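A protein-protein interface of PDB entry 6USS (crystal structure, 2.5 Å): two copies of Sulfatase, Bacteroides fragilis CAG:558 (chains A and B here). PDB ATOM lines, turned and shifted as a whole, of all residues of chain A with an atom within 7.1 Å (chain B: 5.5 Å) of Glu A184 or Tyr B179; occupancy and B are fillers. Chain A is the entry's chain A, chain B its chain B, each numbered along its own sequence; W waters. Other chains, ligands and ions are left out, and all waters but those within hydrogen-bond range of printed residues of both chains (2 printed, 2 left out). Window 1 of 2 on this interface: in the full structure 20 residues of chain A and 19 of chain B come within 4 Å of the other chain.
OH of Tyr A179 lies within hydrogen-bond range of OH of Tyr B179, 3.3 Å away.
The side-chain amino group of Lys A154 is in hydrogen-bond range of the backbone carbonyl oxygen of His B180 (3.1 Å).
The side-chain carboxylate (OE2) of Glu A184 lies within hydrogen-bond range of a ring nitrogen (ND1) of His B180 (2.8 Å).
The side-chain amino group of Lys A154 lies within salt-bridge range of the side-chain carboxylate of Glu B151 (3.7 Å).
The backbone NH (N) of Tyr B179 sits close to the side-chain hydroxyl (OG) of Ser B177 (3.1 Å).
The side-chain hydroxyl (OG) of Ser B177 lies within hydrogen-bond range of the backbone NH (N) of His B180 (3.1 Å).
OE1 of Glu A184 sits at hydrogen-bond distance from ND1 of His A159 (2.8 Å).
The backbone NH of Tyr A179 lies close to the side-chain hydroxyl of Ser A177 (3.2 Å).
The backbone NH (N) of Glu A184 lies within hydrogen-bond range of the backbone carbonyl oxygen (O) of Thr A160, at 2.9 Å.
OE2 of Glu A184 is in salt-bridge range of NZ of Lys A154 (3.5 Å).
Among the printed residues, pairs that only touch across the chains: Asp A155 with Glu B151 (3.6 Å), Tyr A179 with Glu B184 (3.3 Å) and Glu A184 with Tyr B179 (3.4 Å).
Printed residues of chain B within 4 Å of Asp A155: Glu B151 (3.6 Å).
Of the printed residues of chain B, Tyr A179 touches Tyr B179 (3.2 Å) and Glu B184 (3.3 Å).
Of chain B, only Tyr B179 and His B180 come within 4 Å of Glu A184.
Printed residues of chain A within 4 Å of Glu B151: Lys A154 and Asp A155.
Of the printed residues of chain A, His B180 touches Lys A154 and Glu A184.
Met B181 touches none of the printed residues of chain A.
Of the printed residues of chain A, Glu B184 touches Tyr A179.
Of the 20 printed residues of chain A, 4 touch a printed residue of chain B.
Hydrophobic or aromatic side chains of chain A within 4 Å of the printed part of chain B: Tyr A179.
Of the 11 printed residues of chain B, 4 touch a printed residue of chain A.
Hydrophobic or aromatic side chains of chain B that line the printed part of chain A: Tyr B179 and His B180.
Among the printed residues, Asp or Glu carboxylates within 4 Å of a Lys or Arg side-chain nitrogen of the other chain: Lys A154 with Glu B151.
Tyr A179 touches its own counterpart, Tyr B179.
Tyr A179 touches Glu B184, and with the chains exchanged Glu A184 touches Tyr B179.
Of the 7 pairs that touch across the chains among the printed residues, 3 have their exchanged pair printed and touching as well.
Water W1 lies within hydrogen-bond range of O of Glu B184 (2.5 Å) and OG of Ser A177 (2.6 Å).
Water W2 bridges the backbone carbonyl oxygen (O) of Glu A184 (2.6 Å) and the side-chain hydroxyl (OG) of Ser B177 (2.7 Å).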
ATOM      1  N   ALA A 150       7.027 -23.736 -31.350  1.00  0.00           N
ATOM      2  CA  ALA A 150       6.825 -23.418 -29.938  1.00  0.00           C
ATOM      3  C   ALA A 150       5.350 -23.406 -29.563  1.00  0.00           C
ATOM      4  O   ALA A 150       5.006 -23.695 -28.408  1.00  0.00           O
ATOM      5  CB  ALA A 150       7.450 -22.063 -29.597  1.00  0.00           C
ATOM      6  N   LYS A 154       3.880 -25.543 -26.622  1.00  0.00           N
ATOM      7  CA  LYS A 154       3.080 -24.818 -25.631  1.00  0.00           C
ATOM      8  C   LYS A 154       1.694 -25.440 -25.488  1.00  0.00           C
ATOM      9  O   LYS A 154       1.259 -25.771 -24.378  1.00  0.00           O
ATOM     10  CB  LYS A 154       2.986 -23.339 -26.025  1.00  0.00           C
ATOM     11  CG  LYS A 154       2.269 -22.402 -25.033  1.00  0.00           C
ATOM     12  CD  LYS A 154       1.808 -21.100 -25.745  1.00  0.00           C
ATOM     13  CE  LYS A 154       0.379 -20.672 -25.313  1.00  0.00           C
ATOM     14  NZ  LYS A 154       0.159 -20.645 -23.782  1.00  0.00           N
ATOM     15  N   ASP A 155       1.006 -25.657 -26.615  1.00  0.00           N
ATOM     16  CA  ASP A 155      -0.348 -26.192 -26.580  1.00  0.00           C
ATOM     17  C   ASP A 155      -0.401 -27.631 -26.084  1.00  0.00           C
ATOM     18  O   ASP A 155      -1.478 -28.104 -25.707  1.00  0.00           O
ATOM     19  CB  ASP A 155      -0.988 -26.093 -27.966  1.00  0.00           C
ATOM     20  CG  ASP A 155      -1.135 -24.636 -28.465  1.00  0.00           C
ATOM     21  OD1 ASP A 155      -1.226 -23.676 -27.648  1.00  0.00           O
ATOM     22  OD2 ASP A 155      -1.157 -24.457 -29.701  1.00  0.00           O
ATOM     23  N   GLY A 157       1.476 -28.613 -23.427  1.00  0.00           N
ATOM     24  CA  GLY A 157       1.809 -28.600 -22.015  1.00  0.00           C
ATOM     25  C   GLY A 157       3.208 -28.149 -21.660  1.00  0.00           C
ATOM     26  O   GLY A 157       3.531 -28.108 -20.471  1.00  0.00           O
ATOM     27  N   TYR A 158       4.040 -27.787 -22.624  1.00  0.00           N
ATOM     28  CA  TYR A 158       5.382 -27.327 -22.295  1.00  0.00           C
ATOM     29  C   TYR A 158       5.377 -25.862 -21.871  1.00  0.00           C
ATOM     30  O   TYR A 158       4.561 -25.060 -22.337  1.00  0.00           O
ATOM     31  CB  TYR A 158       6.316 -27.522 -23.487  1.00  0.00           C
ATOM     32  CG  TYR A 158       6.940 -28.894 -23.518  1.00  0.00           C
ATOM     33  CD1 TYR A 158       6.181 -30.014 -23.873  1.00  0.00           C
ATOM     34  CD2 TYR A 158       8.285 -29.078 -23.187  1.00  0.00           C
ATOM     35  CE1 TYR A 158       6.741 -31.276 -23.908  1.00  0.00           C
ATOM     36  CE2 TYR A 158       8.854 -30.334 -23.217  1.00  0.00           C
ATOM     37  CZ  TYR A 158       8.080 -31.433 -23.572  1.00  0.00           C
ATOM     38  OH  TYR A 158       8.661 -32.690 -23.592  1.00  0.00           O
ATOM     39  N   HIS A 159       6.283 -25.528 -20.950  1.00  0.00           N
ATOM     40  CA  HIS A 159       6.594 -24.138 -20.623  1.00  0.00           C
ATOM     41  C   HIS A 159       7.726 -23.703 -21.552  1.00  0.00           C
ATOM     42  O   HIS A 159       8.835 -24.244 -21.478  1.00  0.00           O
ATOM     43  CB  HIS A 159       6.983 -23.991 -19.154  1.00  0.00           C
ATOM     44  CG  HIS A 159       7.446 -22.613 -18.785  1.00  0.00           C
ATOM     45  ND1 HIS A 159       6.638 -21.500 -18.893  1.00  0.00           N
ATOM     46  CD2 HIS A 159       8.635 -22.167 -18.311  1.00  0.00           C
ATOM     47  CE1 HIS A 159       7.305 -20.431 -18.491  1.00  0.00           C
ATOM     48  NE2 HIS A 159       8.520 -20.807 -18.133  1.00  0.00           N
ATOM     49  N   THR A 160       7.445 -22.751 -22.448  1.00  0.00           N
ATOM     50  CA  THR A 160       8.341 -22.430 -23.556  1.00  0.00           C
ATOM     51  C   THR A 160       9.089 -21.133 -23.282  1.00  0.00           C
ATOM     52  O   THR A 160       8.468 -20.107 -22.975  1.00  0.00           O
ATOM     53  CB  THR A 160       7.547 -22.310 -24.852  1.00  0.00           C
ATOM     54  OG1 THR A 160       6.483 -21.375 -24.659  1.00  0.00           O
ATOM     55  CG2 THR A 160       6.936 -23.643 -25.206  1.00  0.00           C
ATOM     56  N   ILE A 161      10.412 -21.178 -23.405  1.00  0.00           N
ATOM     57  CA  ILE A 161      11.280 -20.049 -23.095  1.00  0.00           C
ATOM     58  C   ILE A 161      12.147 -19.755 -24.310  1.00  0.00           C
ATOM     59  O   ILE A 161      12.809 -20.662 -24.832  1.00  0.00           O
ATOM     60  CB  ILE A 161      12.184 -20.333 -21.882  1.00  0.00           C
ATOM     61  CG1 ILE A 161      11.365 -20.766 -20.677  1.00  0.00           C
ATOM     62  CG2 ILE A 161      13.054 -19.126 -21.570  1.00  0.00           C
ATOM     63  CD1 ILE A 161      12.200 -21.377 -19.589  1.00  0.00           C
ATOM     64  N   HIS A 162      12.161 -18.488 -24.736  1.00  0.00           N
ATOM     65  CA  HIS A 162      13.091 -17.990 -25.744  1.00  0.00           C
ATOM     66  C   HIS A 162      14.109 -17.038 -25.122  1.00  0.00           C
ATOM     67  O   HIS A 162      13.745 -16.093 -24.401  1.00  0.00           O
ATOM     68  CB  HIS A 162      12.395 -17.250 -26.890  1.00  0.00           C
ATOM     69  CG  HIS A 162      13.360 -16.493 -27.745  1.00  0.00           C
ATOM     70  ND1 HIS A 162      14.083 -17.089 -28.759  1.00  0.00           N
ATOM     71  CD2 HIS A 162      13.817 -15.222 -27.659  1.00  0.00           C
ATOM     72  CE1 HIS A 162      14.895 -16.198 -29.303  1.00  0.00           C
ATOM     73  NE2 HIS A 162      14.754 -15.056 -28.655  1.00  0.00           N
ATOM     74  N   SER A 177       7.889 -11.002 -32.690  1.00  0.00           N
ATOM     75  CA  SER A 177       7.684 -11.295 -31.288  1.00  0.00           C
ATOM     76  C   SER A 177       7.845 -12.779 -31.005  1.00  0.00           C
ATOM     77  O   SER A 177       7.034 -13.583 -31.497  1.00  0.00           O
ATOM     78  CB  SER A 177       6.305 -10.851 -30.852  1.00  0.00           C
ATOM     79  OG  SER A 177       6.114 -11.175 -29.491  1.00  0.00           O
ATOM     80  N   PRO A 178       8.827 -13.186 -30.196  1.00  0.00           N
ATOM     81  CA  PRO A 178       8.809 -14.561 -29.679  1.00  0.00           C
ATOM     82  C   PRO A 178       7.465 -14.953 -29.052  1.00  0.00           C
ATOM     83  O   PRO A 178       7.024 -16.103 -29.212  1.00  0.00           O
ATOM     84  CB  PRO A 178       9.943 -14.545 -28.654  1.00  0.00           C
ATOM     85  CG  PRO A 178      10.877 -13.430 -29.123  1.00  0.00           C
ATOM     86  CD  PRO A 178       9.973 -12.399 -29.695  1.00  0.00           C
ATOM     87  N   TYR A 179       6.793 -14.034 -28.347  1.00  0.00           N
ATOM     88  CA  TYR A 179       5.474 -14.346 -27.795  1.00  0.00           C
ATOM     89  C   TYR A 179       4.488 -14.728 -28.892  1.00  0.00           C
ATOM     90  O   TYR A 179       3.729 -15.694 -28.742  1.00  0.00           O
ATOM     91  CB  TYR A 179       4.917 -13.155 -27.018  1.00  0.00           C
ATOM     92  CG  TYR A 179       5.767 -12.675 -25.878  1.00  0.00           C
ATOM     93  CD1 TYR A 179       5.960 -13.475 -24.745  1.00  0.00           C
ATOM     94  CD2 TYR A 179       6.357 -11.416 -25.919  1.00  0.00           C
ATOM     95  CE1 TYR A 179       6.730 -13.037 -23.684  1.00  0.00           C
ATOM     96  CE2 TYR A 179       7.148 -10.962 -24.864  1.00  0.00           C
ATOM     97  CZ  TYR A 179       7.326 -11.780 -23.747  1.00  0.00           C
ATOM     98  OH  TYR A 179       8.097 -11.347 -22.688  1.00  0.00           O
ATOM     99  N   GLY A 182       4.754 -18.333 -29.988  1.00  0.00           N
ATOM    100  CA  GLY A 182       4.454 -19.411 -29.067  1.00  0.00           C
ATOM    101  C   GLY A 182       5.364 -19.552 -27.861  1.00  0.00           C
ATOM    102  O   GLY A 182       5.239 -20.542 -27.142  1.00  0.00           O
ATOM    103  N   PHE A 183       6.262 -18.604 -27.606  1.00  0.00           N
ATOM    104  CA  PHE A 183       7.075 -18.617 -26.394  1.00  0.00           C
ATOM    105  C   PHE A 183       6.362 -17.865 -25.264  1.00  0.00           C
ATOM    106  O   PHE A 183       5.879 -16.739 -25.453  1.00  0.00           O
ATOM    107  CB  PHE A 183       8.454 -18.002 -26.665  1.00  0.00           C
ATOM    108  CG  PHE A 183       9.353 -18.864 -27.524  1.00  0.00           C
ATOM    109  CD1 PHE A 183      10.137 -19.869 -26.953  1.00  0.00           C
ATOM    110  CD2 PHE A 183       9.413 -18.665 -28.905  1.00  0.00           C
ATOM    111  CE1 PHE A 183      10.978 -20.672 -27.744  1.00  0.00           C
ATOM    112  CE2 PHE A 183      10.244 -19.457 -29.713  1.00  0.00           C
ATOM    113  CZ  PHE A 183      11.028 -20.470 -29.131  1.00  0.00           C
ATOM    114  N   GLU A 184       6.279 -18.497 -24.093  1.00  0.00           N
ATOM    115  CA  GLU A 184       5.657 -17.840 -22.950  1.00  0.00           C
ATOM    116  C   GLU A 184       6.592 -16.852 -22.271  1.00  0.00           C
ATOM    117  O   GLU A 184       6.112 -15.923 -21.606  1.00  0.00           O
ATOM    118  CB  GLU A 184       5.184 -18.888 -21.954  1.00  0.00           C
ATOM    119  CG  GLU A 184       4.126 -19.830 -22.516  1.00  0.00           C
ATOM    120  CD  GLU A 184       3.781 -20.939 -21.543  1.00  0.00           C
ATOM    121  OE1 GLU A 184       4.717 -21.512 -20.941  1.00  0.00           O
ATOM    122  OE2 GLU A 184       2.578 -21.228 -21.366  1.00  0.00           O
ATOM    123  N   VAL A 185       7.906 -17.026 -22.451  1.00  0.00           N
ATOM    124  CA  VAL A 185       8.945 -16.196 -21.851  1.00  0.00           C
ATOM    125  C   VAL A 185       9.901 -15.744 -22.953  1.00  0.00           C
ATOM    126  O   VAL A 185      10.373 -16.568 -23.746  1.00  0.00           O
ATOM    127  CB  VAL A 185       9.710 -16.954 -20.746  1.00  0.00           C
ATOM    128  CG1 VAL A 185      10.909 -16.135 -20.251  1.00  0.00           C
ATOM    129  CG2 VAL A 185       8.769 -17.321 -19.593  1.00  0.00           C
ATOM    130  N   ASN A 186      10.187 -14.438 -22.998  1.00  0.00           N
ATOM    131  CA  ASN A 186      11.089 -13.853 -23.992  1.00  0.00           C
ATOM    132  C   ASN A 186      12.198 -13.084 -23.287  1.00  0.00           C
ATOM    133  O   ASN A 186      11.921 -12.131 -22.554  1.00  0.00           O
ATOM    134  CB  ASN A 186      10.341 -12.919 -24.958  1.00  0.00           C
ATOM    135  CG  ASN A 186      11.281 -12.223 -25.951  1.00  0.00           C
ATOM    136  OD1 ASN A 186      12.432 -12.628 -26.117  1.00  0.00           O
ATOM    137  ND2 ASN A 186      10.780 -11.190 -26.627  1.00  0.00           N
ATOM    138  N   TYR A 249       6.776 -24.589 -11.905  1.00  0.00           N
ATOM    139  CA  TYR A 249       5.612 -25.066 -12.637  1.00  0.00           C
ATOM    140  C   TYR A 249       5.711 -26.563 -12.844  1.00  0.00           C
ATOM    141  O   TYR A 249       6.764 -27.076 -13.248  1.00  0.00           O
ATOM    142  CB  TYR A 249       5.506 -24.385 -13.993  1.00  0.00           C
ATOM    143  CG  TYR A 249       5.416 -22.887 -13.971  1.00  0.00           C
ATOM    144  CD1 TYR A 249       5.102 -22.185 -12.808  1.00  0.00           C
ATOM    145  CD2 TYR A 249       5.615 -22.168 -15.147  1.00  0.00           C
ATOM    146  CE1 TYR A 249       5.008 -20.784 -12.826  1.00  0.00           C
ATOM    147  CE2 TYR A 249       5.511 -20.799 -15.183  1.00  0.00           C
ATOM    148  CZ  TYR A 249       5.215 -20.104 -14.033  1.00  0.00           C
ATOM    149  OH  TYR A 249       5.143 -18.732 -14.113  1.00  0.00           O
ATOM    150  N   GLN A 251       5.245 -28.810 -15.084  1.00  0.00           N
ATOM    151  CA  GLN A 251       5.184 -29.037 -16.525  1.00  0.00           C
ATOM    152  C   GLN A 251       6.615 -29.058 -17.046  1.00  0.00           C
ATOM    153  O   GLN A 251       7.492 -28.421 -16.450  1.00  0.00           O
ATOM    154  CB  GLN A 251       4.360 -27.942 -17.245  1.00  0.00           C
ATOM    155  CG  GLN A 251       4.719 -26.499 -16.869  1.00  0.00           C
ATOM    156  CD  GLN A 251       3.937 -25.428 -17.649  1.00  0.00           C
ATOM    157  OE1 GLN A 251       3.423 -25.671 -18.748  1.00  0.00           O
ATOM    158  NE2 GLN A 251       3.840 -24.237 -17.065  1.00  0.00           N
ATOM    159  N   PRO A 252       6.888 -29.770 -18.136  1.00  0.00           N
ATOM    160  CA  PRO A 252       8.237 -29.735 -18.703  1.00  0.00           C
ATOM    161  C   PRO A 252       8.468 -28.404 -19.396  1.00  0.00           C
ATOM    162  O   PRO A 252       7.534 -27.646 -19.684  1.00  0.00           O
ATOM    163  CB  PRO A 252       8.235 -30.891 -19.701  1.00  0.00           C
ATOM    164  CG  PRO A 252       6.806 -30.971 -20.150  1.00  0.00           C
ATOM    165  CD  PRO A 252       5.944 -30.525 -18.975  1.00  0.00           C
ATOM    166  N   GLU B 151      -6.564 -17.006 -25.408  1.00  0.00           N
ATOM    167  CA  GLU B 151      -5.944 -18.011 -26.267  1.00  0.00           C
ATOM    168  C   GLU B 151      -6.797 -18.272 -27.497  1.00  0.00           C
ATOM    169  O   GLU B 151      -6.286 -18.329 -28.622  1.00  0.00           O
ATOM    170  CB  GLU B 151      -5.721 -19.308 -25.498  1.00  0.00           C
ATOM    171  CG  GLU B 151      -4.951 -20.354 -26.300  1.00  0.00           C
ATOM    172  CD  GLU B 151      -3.446 -20.070 -26.332  1.00  0.00           C
ATOM    173  OE1 GLU B 151      -2.925 -19.421 -25.372  1.00  0.00           O
ATOM    174  OE2 GLU B 151      -2.792 -20.490 -27.319  1.00  0.00           O
ATOM    175  N   SER B 177       1.044 -15.651 -15.412  1.00  0.00           N
ATOM    176  CA  SER B 177       1.556 -14.979 -16.598  1.00  0.00           C
ATOM    177  C   SER B 177       0.445 -14.706 -17.595  1.00  0.00           C
ATOM    178  O   SER B 177      -0.125 -15.667 -18.138  1.00  0.00           O
ATOM    179  CB  SER B 177       2.631 -15.824 -17.264  1.00  0.00           C
ATOM    180  OG  SER B 177       2.948 -15.284 -18.536  1.00  0.00           O
ATOM    181  N   PRO B 178       0.129 -13.439 -17.895  1.00  0.00           N
ATOM    182  CA  PRO B 178      -0.764 -13.160 -19.037  1.00  0.00           C
ATOM    183  C   PRO B 178      -0.313 -13.814 -20.331  1.00  0.00           C
ATOM    184  O   PRO B 178      -1.162 -14.177 -21.160  1.00  0.00           O
ATOM    185  CB  PRO B 178      -0.733 -11.632 -19.135  1.00  0.00           C
ATOM    186  CG  PRO B 178      -0.490 -11.185 -17.697  1.00  0.00           C
ATOM    187  CD  PRO B 178       0.448 -12.219 -17.122  1.00  0.00           C
ATOM    188  N   TYR B 179       0.997 -13.990 -20.534  1.00  0.00           N
ATOM    189  CA  TYR B 179       1.455 -14.704 -21.723  1.00  0.00           C
ATOM    190  C   TYR B 179       0.991 -16.157 -21.707  1.00  0.00           C
ATOM    191  O   TYR B 179       0.496 -16.671 -22.716  1.00  0.00           O
ATOM    192  CB  TYR B 179       2.971 -14.660 -21.836  1.00  0.00           C
ATOM    193  CG  TYR B 179       3.573 -13.291 -21.896  1.00  0.00           C
ATOM    194  CD1 TYR B 179       3.381 -12.470 -23.009  1.00  0.00           C
ATOM    195  CD2 TYR B 179       4.386 -12.828 -20.853  1.00  0.00           C
ATOM    196  CE1 TYR B 179       3.976 -11.209 -23.080  1.00  0.00           C
ATOM    197  CE2 TYR B 179       4.985 -11.573 -20.906  1.00  0.00           C
ATOM    198  CZ  TYR B 179       4.771 -10.764 -22.022  1.00  0.00           C
ATOM    199  OH  TYR B 179       5.359  -9.519 -22.073  1.00  0.00           O
ATOM    200  N   HIS B 180       1.163 -16.847 -20.573  1.00  0.00           N
ATOM    201  CA  HIS B 180       0.672 -18.217 -20.495  1.00  0.00           C
ATOM    202  C   HIS B 180      -0.811 -18.297 -20.811  1.00  0.00           C
ATOM    203  O   HIS B 180      -1.282 -19.313 -21.332  1.00  0.00           O
ATOM    204  CB  HIS B 180       0.909 -18.819 -19.116  1.00  0.00           C
ATOM    205  CG  HIS B 180       0.160 -20.097 -18.911  1.00  0.00           C
ATOM    206  ND1 HIS B 180       0.609 -21.306 -19.402  1.00  0.00           N
ATOM    207  CD2 HIS B 180      -1.045 -20.344 -18.342  1.00  0.00           C
ATOM    208  CE1 HIS B 180      -0.276 -22.247 -19.118  1.00  0.00           C
ATOM    209  NE2 HIS B 180      -1.291 -21.691 -18.480  1.00  0.00           N
ATOM    210  N   MET B 181      -1.559 -17.240 -20.496  1.00  0.00           N
ATOM    211  CA  MET B 181      -3.002 -17.191 -20.692  1.00  0.00           C
ATOM    212  C   MET B 181      -3.412 -16.719 -22.090  1.00  0.00           C
ATOM    213  O   MET B 181      -4.602 -16.470 -22.325  1.00  0.00           O
ATOM    214  CB  MET B 181      -3.633 -16.302 -19.619  1.00  0.00           C
ATOM    215  CG  MET B 181      -3.393 -16.852 -18.233  1.00  0.00           C
ATOM    216  SD  MET B 181      -4.402 -18.306 -17.934  1.00  0.00           S
ATOM    217  CE  MET B 181      -6.038 -17.557 -17.816  1.00  0.00           C
ATOM    218  N   GLY B 182      -2.463 -16.597 -23.019  1.00  0.00           N
ATOM    219  CA  GLY B 182      -2.784 -16.322 -24.403  1.00  0.00           C
ATOM    220  C   GLY B 182      -2.637 -14.882 -24.836  1.00  0.00           C
ATOM    221  O   GLY B 182      -2.955 -14.567 -25.987  1.00  0.00           O
ATOM    222  N   PHE B 183      -2.177 -14.002 -23.967  1.00  0.00           N
ATOM    223  CA  PHE B 183      -1.899 -12.637 -24.374  1.00  0.00           C
ATOM    224  C   PHE B 183      -0.530 -12.559 -25.029  1.00  0.00           C
ATOM    225  O   PHE B 183       0.450 -13.078 -24.483  1.00  0.00           O
ATOM    226  CB  PHE B 183      -1.962 -11.707 -23.162  1.00  0.00           C
ATOM    227  CG  PHE B 183      -3.353 -11.433 -22.702  1.00  0.00           C
ATOM    228  CD1 PHE B 183      -4.195 -10.613 -23.445  1.00  0.00           C
ATOM    229  CD2 PHE B 183      -3.836 -12.020 -21.545  1.00  0.00           C
ATOM    230  CE1 PHE B 183      -5.480 -10.370 -23.027  1.00  0.00           C
ATOM    231  CE2 PHE B 183      -5.128 -11.779 -21.120  1.00  0.00           C
ATOM    232  CZ  PHE B 183      -5.949 -10.957 -21.860  1.00  0.00           C
ATOM    233  N   GLU B 184      -0.454 -11.887 -26.186  1.00  0.00           N
ATOM    234  CA  GLU B 184       0.826 -11.724 -26.877  1.00  0.00           C
ATOM    235  C   GLU B 184       1.644 -10.563 -26.334  1.00  0.00           C
ATOM    236  O   GLU B 184       2.868 -10.569 -26.469  1.00  0.00           O
ATOM    237  CB  GLU B 184       0.620 -11.507 -28.373  1.00  0.00           C
ATOM    238  CG  GLU B 184       0.201 -12.728 -29.151  1.00  0.00           C
ATOM    239  CD  GLU B 184      -0.248 -12.368 -30.561  1.00  0.00           C
ATOM    240  OE1 GLU B 184      -0.158 -13.218 -31.464  1.00  0.00           O
ATOM    241  OE2 GLU B 184      -0.692 -11.224 -30.766  1.00  0.00           O
ATOM    242  N   VAL B 185       0.995  -9.554 -25.761  1.00  0.00           N
ATOM    243  CA  VAL B 185       1.657  -8.421 -25.122  1.00  0.00           C
ATOM    244  C   VAL B 185       1.138  -8.308 -23.688  1.00  0.00           C
ATOM    245  O   VAL B 185      -0.069  -8.451 -23.445  1.00  0.00           O
ATOM    246  CB  VAL B 185       1.415  -7.103 -25.901  1.00  0.00           C
ATOM    247  CG1 VAL B 185       2.040  -5.929 -25.168  1.00  0.00           C
ATOM    248  CG2 VAL B 185       1.961  -7.190 -27.348  1.00  0.00           C
ATOM    249  N   ASN B 186       2.042  -8.041 -22.739  1.00  0.00           N
ATOM    250  CA  ASN B 186       1.679  -7.895 -21.330  1.00  0.00           C
ATOM    251  C   ASN B 186       2.290  -6.621 -20.771  1.00  0.00           C
ATOM    252  O   ASN B 186       3.516  -6.488 -20.733  1.00  0.00           O
ATOM    253  CB  ASN B 186       2.145  -9.094 -20.504  1.00  0.00           C
ATOM    254  CG  ASN B 186       1.986  -8.868 -19.001  1.00  0.00           C
ATOM    255  OD1 ASN B 186       1.179  -8.037 -18.563  1.00  0.00           O
ATOM    256  ND2 ASN B 186       2.744  -9.621 -18.203  1.00  0.00           N
HETATM  257  O   HOH W   1       4.590  -9.593 -28.057  1.00  0.00           O
HETATM  258  O   HOH W   2       5.521 -15.541 -19.132  1.00  0.00           O
